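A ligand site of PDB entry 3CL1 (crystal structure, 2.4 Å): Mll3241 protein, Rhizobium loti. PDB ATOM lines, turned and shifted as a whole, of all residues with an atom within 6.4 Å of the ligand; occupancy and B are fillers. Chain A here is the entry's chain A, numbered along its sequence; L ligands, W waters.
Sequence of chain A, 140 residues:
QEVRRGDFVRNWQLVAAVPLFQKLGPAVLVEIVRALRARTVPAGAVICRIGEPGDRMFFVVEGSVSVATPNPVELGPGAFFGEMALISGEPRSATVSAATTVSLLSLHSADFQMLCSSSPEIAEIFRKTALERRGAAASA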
ATOM      1  N   CYS A  48      -1.883 -21.135 -27.107  1.00  0.00           N
ATOM      2  CA  CYS A  48      -1.213 -22.166 -27.869  1.00  0.00           C
ATOM      3  C   CYS A  48      -1.287 -21.864 -29.353  1.00  0.00           C
ATOM      4  O   CYS A  48      -2.201 -21.192 -29.820  1.00  0.00           O
ATOM      5  CB  CYS A  48      -1.730 -23.558 -27.519  1.00  0.00           C
ATOM      6  SG  CYS A  48      -3.457 -23.855 -27.806  1.00  0.00           S
ATOM      7  N   GLY A  54       1.776 -30.078 -28.261  1.00  0.00           N
ATOM      8  CA  GLY A  54       0.949 -29.798 -27.094  1.00  0.00           C
ATOM      9  C   GLY A  54       1.197 -30.805 -25.994  1.00  0.00           C
ATOM     10  O   GLY A  54       1.061 -32.003 -26.215  1.00  0.00           O
ATOM     11  N   ARG A  56      -0.143 -29.974 -22.752  1.00  0.00           N
ATOM     12  CA  ARG A  56      -1.154 -29.642 -21.757  1.00  0.00           C
ATOM     13  C   ARG A  56      -2.499 -29.227 -22.336  1.00  0.00           C
ATOM     14  O   ARG A  56      -2.621 -28.889 -23.517  1.00  0.00           O
ATOM     15  CB  ARG A  56      -0.645 -28.587 -20.776  1.00  0.00           C
ATOM     16  CG  ARG A  56      -0.616 -27.187 -21.299  1.00  0.00           C
ATOM     17  CD  ARG A  56       0.368 -26.379 -20.501  1.00  0.00           C
ATOM     18  NE  ARG A  56       1.726 -26.762 -20.851  1.00  0.00           N
ATOM     19  CZ  ARG A  56       2.822 -26.363 -20.215  1.00  0.00           C
ATOM     20  NH1 ARG A  56       2.717 -25.554 -19.166  1.00  0.00           N
ATOM     21  NH2 ARG A  56       4.015 -26.777 -20.625  1.00  0.00           N
ATOM     22  N   MET A  57      -3.528 -29.266 -21.507  1.00  0.00           N
ATOM     23  CA  MET A  57      -4.839 -28.828 -21.917  1.00  0.00           C
ATOM     24  C   MET A  57      -5.319 -27.784 -20.920  1.00  0.00           C
ATOM     25  O   MET A  57      -4.768 -27.660 -19.830  1.00  0.00           O
ATOM     26  CB  MET A  57      -5.798 -30.003 -21.999  1.00  0.00           C
ATOM     27  CG  MET A  57      -6.386 -30.407 -20.695  1.00  0.00           C
ATOM     28  SD  MET A  57      -8.017 -31.045 -21.012  1.00  0.00           S
ATOM     29  CE  MET A  57      -8.737 -29.901 -22.172  1.00  0.00           C
ATOM     30  N   VAL A  67     -10.455 -19.437 -30.676  1.00  0.00           N
ATOM     31  CA  VAL A  67      -9.839 -20.491 -31.450  1.00  0.00           C
ATOM     32  C   VAL A  67      -9.775 -20.047 -32.887  1.00  0.00           C
ATOM     33  O   VAL A  67     -10.813 -19.872 -33.526  1.00  0.00           O
ATOM     34  CB  VAL A  67     -10.614 -21.832 -31.331  1.00  0.00           C
ATOM     35  CG1 VAL A  67      -9.909 -22.939 -32.106  1.00  0.00           C
ATOM     36  CG2 VAL A  67     -10.783 -22.217 -29.869  1.00  0.00           C
ATOM     37  N   THR A  69      -9.798 -20.965 -35.836  1.00  0.00           N
ATOM     38  CA  THR A  69     -10.242 -21.796 -36.957  1.00  0.00           C
ATOM     39  C   THR A  69     -10.666 -20.844 -38.084  1.00  0.00           C
ATOM     40  O   THR A  69     -10.856 -19.636 -37.823  1.00  0.00           O
ATOM     41  CB  THR A  69     -11.422 -22.707 -36.518  1.00  0.00           C
ATOM     42  OG1 THR A  69     -12.340 -21.954 -35.718  1.00  0.00           O
ATOM     43  CG2 THR A  69     -10.933 -23.903 -35.710  1.00  0.00           C
ATOM     44  N   VAL A  73     -13.717 -19.613 -33.133  1.00  0.00           N
ATOM     45  CA  VAL A  73     -14.608 -20.106 -32.085  1.00  0.00           C
ATOM     46  C   VAL A  73     -14.223 -19.460 -30.764  1.00  0.00           C
ATOM     47  O   VAL A  73     -13.088 -19.578 -30.310  1.00  0.00           O
ATOM     48  CB  VAL A  73     -14.578 -21.655 -31.979  1.00  0.00           C
ATOM     49  CG1 VAL A  73     -15.498 -22.134 -30.897  1.00  0.00           C
ATOM     50  CG2 VAL A  73     -14.962 -22.291 -33.314  1.00  0.00           C
ATOM     51  N   LEU A  75     -14.491 -19.537 -26.834  1.00  0.00           N
ATOM     52  CA  LEU A  75     -14.802 -20.415 -25.694  1.00  0.00           C
ATOM     53  C   LEU A  75     -14.850 -19.655 -24.369  1.00  0.00           C
ATOM     54  O   LEU A  75     -13.919 -18.925 -24.054  1.00  0.00           O
ATOM     55  CB  LEU A  75     -13.815 -21.589 -25.597  1.00  0.00           C
ATOM     56  CG  LEU A  75     -13.647 -22.484 -26.836  1.00  0.00           C
ATOM     57  CD1 LEU A  75     -12.518 -23.466 -26.591  1.00  0.00           C
ATOM     58  CD2 LEU A  75     -14.929 -23.210 -27.235  1.00  0.00           C
ATOM     59  N   PHE A  80     -13.178 -26.108 -22.166  1.00  0.00           N
ATOM     60  CA  PHE A  80     -11.831 -26.651 -22.173  1.00  0.00           C
ATOM     61  C   PHE A  80     -11.314 -26.711 -23.598  1.00  0.00           C
ATOM     62  O   PHE A  80     -12.099 -26.831 -24.548  1.00  0.00           O
ATOM     63  CB  PHE A  80     -11.778 -28.030 -21.513  1.00  0.00           C
ATOM     64  CG  PHE A  80     -12.666 -29.055 -22.156  1.00  0.00           C
ATOM     65  CD1 PHE A  80     -12.276 -29.703 -23.329  1.00  0.00           C
ATOM     66  CD2 PHE A  80     -13.887 -29.379 -21.593  1.00  0.00           C
ATOM     67  CE1 PHE A  80     -13.109 -30.628 -23.945  1.00  0.00           C
ATOM     68  CE2 PHE A  80     -14.722 -30.324 -22.180  1.00  0.00           C
ATOM     69  CZ  PHE A  80     -14.328 -30.949 -23.373  1.00  0.00           C
ATOM     70  N   PHE A  81     -10.000 -26.599 -23.747  1.00  0.00           N
ATOM     71  CA  PHE A  81      -9.366 -26.685 -25.070  1.00  0.00           C
ATOM     72  C   PHE A  81      -7.958 -27.271 -24.956  1.00  0.00           C
ATOM     73  O   PHE A  81      -7.410 -27.330 -23.875  1.00  0.00           O
ATOM     74  CB  PHE A  81      -9.369 -25.319 -25.769  1.00  0.00           C
ATOM     75  CG  PHE A  81      -8.582 -24.267 -25.047  1.00  0.00           C
ATOM     76  CD1 PHE A  81      -7.241 -24.051 -25.348  1.00  0.00           C
ATOM     77  CD2 PHE A  81      -9.171 -23.485 -24.061  1.00  0.00           C
ATOM     78  CE1 PHE A  81      -6.502 -23.089 -24.680  1.00  0.00           C
ATOM     79  CE2 PHE A  81      -8.443 -22.515 -23.383  1.00  0.00           C
ATOM     80  CZ  PHE A  81      -7.107 -22.306 -23.702  1.00  0.00           C
ATOM     81  N   GLY A  82      -7.393 -27.726 -26.075  1.00  0.00           N
ATOM     82  CA  GLY A  82      -6.059 -28.319 -26.115  1.00  0.00           C
ATOM     83  C   GLY A  82      -6.032 -29.833 -25.945  1.00  0.00           C
ATOM     84  O   GLY A  82      -4.963 -30.447 -25.982  1.00  0.00           O
ATOM     85  N   GLU A  83      -7.212 -30.432 -25.772  1.00  0.00           N
ATOM     86  CA  GLU A  83      -7.346 -31.873 -25.579  1.00  0.00           C
ATOM     87  C   GLU A  83      -6.989 -32.669 -26.844  1.00  0.00           C
ATOM     88  O   GLU A  83      -6.550 -33.812 -26.750  1.00  0.00           O
ATOM     89  CB  GLU A  83      -8.778 -32.232 -25.130  1.00  0.00           C
ATOM     90  CG  GLU A  83      -9.868 -32.117 -26.224  1.00  0.00           C
ATOM     91  CD  GLU A  83     -10.179 -30.680 -26.649  1.00  0.00           C
ATOM     92  OE1 GLU A  83     -10.008 -29.747 -25.818  1.00  0.00           O
ATOM     93  OE2 GLU A  83     -10.601 -30.487 -27.807  1.00  0.00           O
ATOM     94  N   MET A  84      -7.201 -32.061 -28.015  1.00  0.00           N
ATOM     95  CA  MET A  84      -6.975 -32.780 -29.266  1.00  0.00           C
ATOM     96  C   MET A  84      -5.537 -33.242 -29.442  1.00  0.00           C
ATOM     97  O   MET A  84      -5.314 -34.376 -29.846  1.00  0.00           O
ATOM     98  CB  MET A  84      -7.413 -31.948 -30.466  1.00  0.00           C
ATOM     99  CG  MET A  84      -8.896 -31.947 -30.689  1.00  0.00           C
ATOM    100  SD  MET A  84      -9.409 -30.676 -31.856  1.00  0.00           S
ATOM    101  CE  MET A  84      -8.686 -31.278 -33.384  1.00  0.00           C
ATOM    102  N   ALA A  85      -4.578 -32.380 -29.094  1.00  0.00           N
ATOM    103  CA  ALA A  85      -3.160 -32.759 -29.155  1.00  0.00           C
ATOM    104  C   ALA A  85      -2.801 -33.833 -28.132  1.00  0.00           C
ATOM    105  O   ALA A  85      -1.926 -34.662 -28.384  1.00  0.00           O
ATOM    106  CB  ALA A  85      -2.252 -31.522 -28.973  1.00  0.00           C
ATOM    107  N   LEU A  86      -3.463 -33.824 -26.971  1.00  0.00           N
ATOM    108  CA  LEU A  86      -3.179 -34.794 -25.913  1.00  0.00           C
ATOM    109  C   LEU A  86      -3.708 -36.181 -26.270  1.00  0.00           C
ATOM    110  O   LEU A  86      -3.069 -37.181 -25.980  1.00  0.00           O
ATOM    111  CB  LEU A  86      -3.735 -34.330 -24.560  1.00  0.00           C
ATOM    112  CG  LEU A  86      -3.152 -33.037 -23.964  1.00  0.00           C
ATOM    113  CD1 LEU A  86      -3.611 -32.824 -22.553  1.00  0.00           C
ATOM    114  CD2 LEU A  86      -1.663 -33.047 -24.022  1.00  0.00           C
ATOM    115  N   GLU A  90      -0.884 -35.341 -32.057  1.00  0.00           N
ATOM    116  CA  GLU A  90      -0.578 -34.421 -33.156  1.00  0.00           C
ATOM    117  C   GLU A  90      -0.290 -33.006 -32.646  1.00  0.00           C
ATOM    118  O   GLU A  90      -0.608 -32.704 -31.506  1.00  0.00           O
ATOM    119  CB  GLU A  90      -1.740 -34.413 -34.153  1.00  0.00           C
ATOM    120  CG  GLU A  90      -2.038 -35.786 -34.720  1.00  0.00           C
ATOM    121  CD  GLU A  90      -3.275 -35.833 -35.592  1.00  0.00           C
ATOM    122  OE1 GLU A  90      -4.090 -34.893 -35.546  1.00  0.00           O
ATOM    123  OE2 GLU A  90      -3.431 -36.832 -36.326  1.00  0.00           O
ATOM    124  N   PRO A  91       0.302 -32.129 -33.491  1.00  0.00           N
ATOM    125  CA  PRO A  91       0.527 -30.738 -33.076  1.00  0.00           C
ATOM    126  C   PRO A  91      -0.789 -29.978 -32.927  1.00  0.00           C
ATOM    127  O   PRO A  91      -1.811 -30.418 -33.467  1.00  0.00           O
ATOM    128  CB  PRO A  91       1.305 -30.144 -34.265  1.00  0.00           C
ATOM    129  CG  PRO A  91       1.796 -31.291 -35.053  1.00  0.00           C
ATOM    130  CD  PRO A  91       0.780 -32.370 -34.863  1.00  0.00           C
ATOM    131  N   ARG A  92      -0.782 -28.841 -32.229  1.00  0.00           N
ATOM    132  CA  ARG A  92      -1.976 -28.010 -32.100  1.00  0.00           C
ATOM    133  C   ARG A  92      -2.612 -27.803 -33.464  1.00  0.00           C
ATOM    134  O   ARG A  92      -1.926 -27.466 -34.419  1.00  0.00           O
ATOM    135  CB  ARG A  92      -1.659 -26.649 -31.479  1.00  0.00           C
ATOM    136  CG  ARG A  92      -0.990 -26.716 -30.119  1.00  0.00           C
ATOM    137  CD  ARG A  92      -1.849 -27.445 -29.091  1.00  0.00           C
ATOM    138  NE  ARG A  92      -1.328 -27.257 -27.735  1.00  0.00           N
ATOM    139  CZ  ARG A  92      -1.836 -27.827 -26.650  1.00  0.00           C
ATOM    140  NH1 ARG A  92      -2.873 -28.642 -26.725  1.00  0.00           N
ATOM    141  NH2 ARG A  92      -1.287 -27.576 -25.464  1.00  0.00           N
ATOM    142  N   SER A  93      -3.931 -28.006 -33.553  1.00  0.00           N
ATOM    143  CA  SER A  93      -4.654 -27.891 -34.809  1.00  0.00           C
ATOM    144  C   SER A  93      -5.052 -26.453 -35.095  1.00  0.00           C
ATOM    145  O   SER A  93      -5.448 -26.116 -36.213  1.00  0.00           O
ATOM    146  CB  SER A  93      -5.899 -28.767 -34.793  1.00  0.00           C
ATOM    147  OG  SER A  93      -6.741 -28.431 -33.707  1.00  0.00           O
ATOM    148  N   ALA A  94      -4.969 -25.602 -34.061  1.00  0.00           N
ATOM    149  CA  ALA A  94      -5.381 -24.216 -34.161  1.00  0.00           C
ATOM    150  C   ALA A  94      -4.681 -23.372 -33.105  1.00  0.00           C
ATOM    151  O   ALA A  94      -4.276 -23.875 -32.060  1.00  0.00           O
ATOM    152  CB  ALA A  94      -6.885 -24.096 -33.998  1.00  0.00           C
ATOM    153  N   THR A  95      -4.517 -22.090 -33.399  1.00  0.00           N
ATOM    154  CA  THR A  95      -4.051 -21.124 -32.430  1.00  0.00           C
ATOM    155  C   THR A  95      -5.223 -20.713 -31.546  1.00  0.00           C
ATOM    156  O   THR A  95      -6.338 -20.515 -32.023  1.00  0.00           O
ATOM    157  CB  THR A  95      -3.414 -19.926 -33.140  1.00  0.00           C
ATOM    158  OG1 THR A  95      -2.186 -20.346 -33.730  1.00  0.00           O
ATOM    159  CG2 THR A  95      -3.120 -18.788 -32.161  1.00  0.00           C
ATOM    160  N   VAL A  96      -4.963 -20.654 -30.256  1.00  0.00           N
ATOM    161  CA  VAL A  96      -5.938 -20.189 -29.295  1.00  0.00           C
ATOM    162  C   VAL A  96      -5.296 -18.982 -28.607  1.00  0.00           C
ATOM    163  O   VAL A  96      -4.182 -19.077 -28.090  1.00  0.00           O
ATOM    164  CB  VAL A  96      -6.302 -21.285 -28.239  1.00  0.00           C
ATOM    165  CG1 VAL A  96      -7.380 -20.781 -27.301  1.00  0.00           C
ATOM    166  CG2 VAL A  96      -6.737 -22.575 -28.913  1.00  0.00           C
ATOM    167  N   GLU A 132     -15.920 -34.016 -32.386  1.00  0.00           N
ATOM    168  CA  GLU A 132     -16.791 -32.946 -32.854  1.00  0.00           C
ATOM    169  C   GLU A 132     -15.959 -31.792 -33.441  1.00  0.00           C
ATOM    170  O   GLU A 132     -16.265 -31.295 -34.518  1.00  0.00           O
ATOM    171  CB  GLU A 132     -17.660 -32.423 -31.710  1.00  0.00           C
ATOM    172  CG  GLU A 132     -18.781 -33.319 -31.258  1.00  0.00           C
ATOM    173  CD  GLU A 132     -19.737 -32.613 -30.291  1.00  0.00           C
ATOM    174  OE1 GLU A 132     -20.890 -32.327 -30.693  1.00  0.00           O
ATOM    175  OE2 GLU A 132     -19.338 -32.330 -29.136  1.00  0.00           O
ATOM    176  N   ARG A 133     -14.911 -31.392 -32.718  1.00  0.00           N
ATOM    177  CA  ARG A 133     -14.041 -30.291 -33.110  1.00  0.00           C
ATOM    178  C   ARG A 133     -13.218 -30.602 -34.352  1.00  0.00           C
ATOM    179  O   ARG A 133     -13.048 -29.738 -35.215  1.00  0.00           O
ATOM    180  CB  ARG A 133     -13.147 -29.876 -31.932  1.00  0.00           C
ATOM    181  CG  ARG A 133     -13.894 -29.104 -30.874  1.00  0.00           C
ATOM    182  CD  ARG A 133     -13.142 -28.974 -29.561  1.00  0.00           C
ATOM    183  NE  ARG A 133     -13.937 -28.163 -28.625  1.00  0.00           N
ATOM    184  CZ  ARG A 133     -13.600 -27.851 -27.380  1.00  0.00           C
ATOM    185  NH1 ARG A 133     -12.454 -28.285 -26.868  1.00  0.00           N
ATOM    186  NH2 ARG A 133     -14.409 -27.104 -26.646  1.00  0.00           N
ATOM    187  N   ARG A 134     -12.715 -31.828 -34.439  1.00  0.00           N
ATOM    188  CA  ARG A 134     -11.941 -32.284 -35.607  1.00  0.00           C
ATOM    189  C   ARG A 134     -12.817 -32.357 -36.858  1.00  0.00           C
ATOM    190  O   ARG A 134     -13.964 -32.819 -36.807  1.00  0.00           O
ATOM    191  CB  ARG A 134     -11.274 -33.631 -35.341  1.00  0.00           C
HETATM  192  P1  LIG L   1      -5.482 -28.722 -29.944  1.00  0.00           P
HETATM  193  O1  LIG L   1      -5.484 -29.179 -31.378  1.00  0.00           O
HETATM  194  O2  LIG L   1      -4.554 -29.408 -28.976  1.00  0.00           O
HETATM  195  O3  LIG L   1      -5.130 -27.120 -29.908  1.00  0.00           O
HETATM  196  C1  LIG L   1      -6.051 -26.134 -30.398  1.00  0.00           C
HETATM  197  C2  LIG L   1      -7.372 -26.405 -29.690  1.00  0.00           C
HETATM  198  O4  LIG L   1      -8.494 -25.617 -30.075  1.00  0.00           O
HETATM  199  C3  LIG L   1      -7.877 -27.819 -29.912  1.00  0.00           C
HETATM  200  O5  LIG L   1      -6.972 -28.747 -29.329  1.00  0.00           O
HETATM  201  C4  LIG L   1      -9.274 -27.729 -29.306  1.00  0.00           C
HETATM  202  O6  LIG L   1      -9.235 -28.059 -27.911  1.00  0.00           O
HETATM  203  C5  LIG L   1      -9.627 -26.253 -29.495  1.00  0.00           C
HETATM  204  N1  LIG L   1     -10.779 -26.140 -30.423  1.00  0.00           N
HETATM  205  C6  LIG L   1     -11.985 -25.651 -30.125  1.00  0.00           C
HETATM  206  N2  LIG L   1     -12.810 -25.702 -31.199  1.00  0.00           N
HETATM  207  C7  LIG L   1     -12.113 -26.232 -32.214  1.00  0.00           C
HETATM  208  C8  LIG L   1     -12.383 -26.576 -33.627  1.00  0.00           C
HETATM  209  O7  LIG L   1     -13.508 -26.352 -34.122  1.00  0.00           O
HETATM  210  N3  LIG L   1     -11.378 -27.115 -34.350  1.00  0.00           N
HETATM  211  C9  LIG L   1     -10.165 -27.359 -33.814  1.00  0.00           C
HETATM  212  N4  LIG L   1      -9.197 -27.906 -34.580  1.00  0.00           N
HETATM  213  N5  LIG L   1      -9.855 -27.079 -32.529  1.00  0.00           N
HETATM  214  C10 LIG L   1     -10.776 -26.524 -31.700  1.00  0.00           C
HETATM  215  O   HOH W   1      -4.242 -31.625 -32.415  1.00  0.00           O
HETATM  216  O   HOH W   2     -13.832 -25.209 -37.408  1.00  0.00           O
HETATM  217  O   HOH W   3     -15.483 -25.567 -31.098  1.00  0.00           O
HETATM  218  O   HOH W   4     -16.344 -26.164 -33.370  1.00  0.00           O
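The side-chain sulfur (SD) of Met 84 lies close to a nitrogen (N5) of the ligand, at 3.7 Å. CG1 of Val 67 touches O4 of the ligand (3.6 Å). CG2 of Thr 69 touches N3 of the ligand, 3.5 Å away. Phe 81 touches the ligand (CA to O6, 3.2 Å). O of Ala 94 touches C1 of the ligand, 3.3 Å away. CG2 of Val 96 touches O4 of the ligand, at 3.7 Å. Within 4 Å of the ligand: Val 67, Thr 69, Phe 81, Gly 82, Glu 83, Met 84, Ala 85, Arg 92, Ser 93, Ala 94, Val 96 and Arg 133.
The guanidinium group (NH1) of Arg 92 is in salt-bridge range of an oxygen (O2) of the ligand, at 2.9 Å. N of Ala 85 sits at hydrogen-bond distance from O2 of the ligand (3.0 Å). The backbone NH (N) of Gly 82 lies within hydrogen-bond range of an oxygen (O6) of the ligand. N4 of the ligand lies within hydrogen-bond range of OG of Ser 93, at 2.7 Å. The side-chain carboxylate of Glu 83 lies within hydrogen-bond range of an oxygen (O6) of the ligand (2.8 Å). The guanidinium group (NH1) of Arg 133 is in hydrogen-bond range of an oxygen (O6) of the ligand (3.4 Å). The backbone NH (N) of Ser 93 lies within hydrogen-bond range of an oxygen (O1) of the ligand, at 2.9 Å. The backbone carbonyl oxygen (O) of Arg 133 sits at hydrogen-bond distance from a nitrogen (N3) of the ligand, at 3.2 Å.
Water W1 lies within hydrogen-bond range of the backbone carbonyl oxygen (O) of Pro 91, an oxygen (O1) of the ligand and the backbone NH (N) of Ala 85.
The side-chain hydroxyl (OG1) of Thr 69 lies within hydrogen-bond range of the backbone carbonyl oxygen (O) of Val 67, 3.4 Å away. The side-chain carboxylate (OE2) of Glu 83 lies within salt-bridge range of the guanidinium group (NH1) of Arg 133 (3.0 Å). N of Val 67 lies within hydrogen-bond range of O of Val 73 (2.7 Å). The guanidinium group (NH2) of Arg 92 is in hydrogen-bond range of the backbone carbonyl oxygen (O) of Arg 56, 2.7 Å away. The backbone carbonyl oxygen (O) of Phe 80 sits at hydrogen-bond distance from the guanidinium group (NH1) of Arg 133 (2.8 Å). The backbone carbonyl oxygen (O) of Cys 48 is in hydrogen-bond range of the backbone NH (N) of Val 96 (2.8 Å). O of Gly 82 is in hydrogen-bond range of NH1 of Arg 92, at 2.9 Å.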
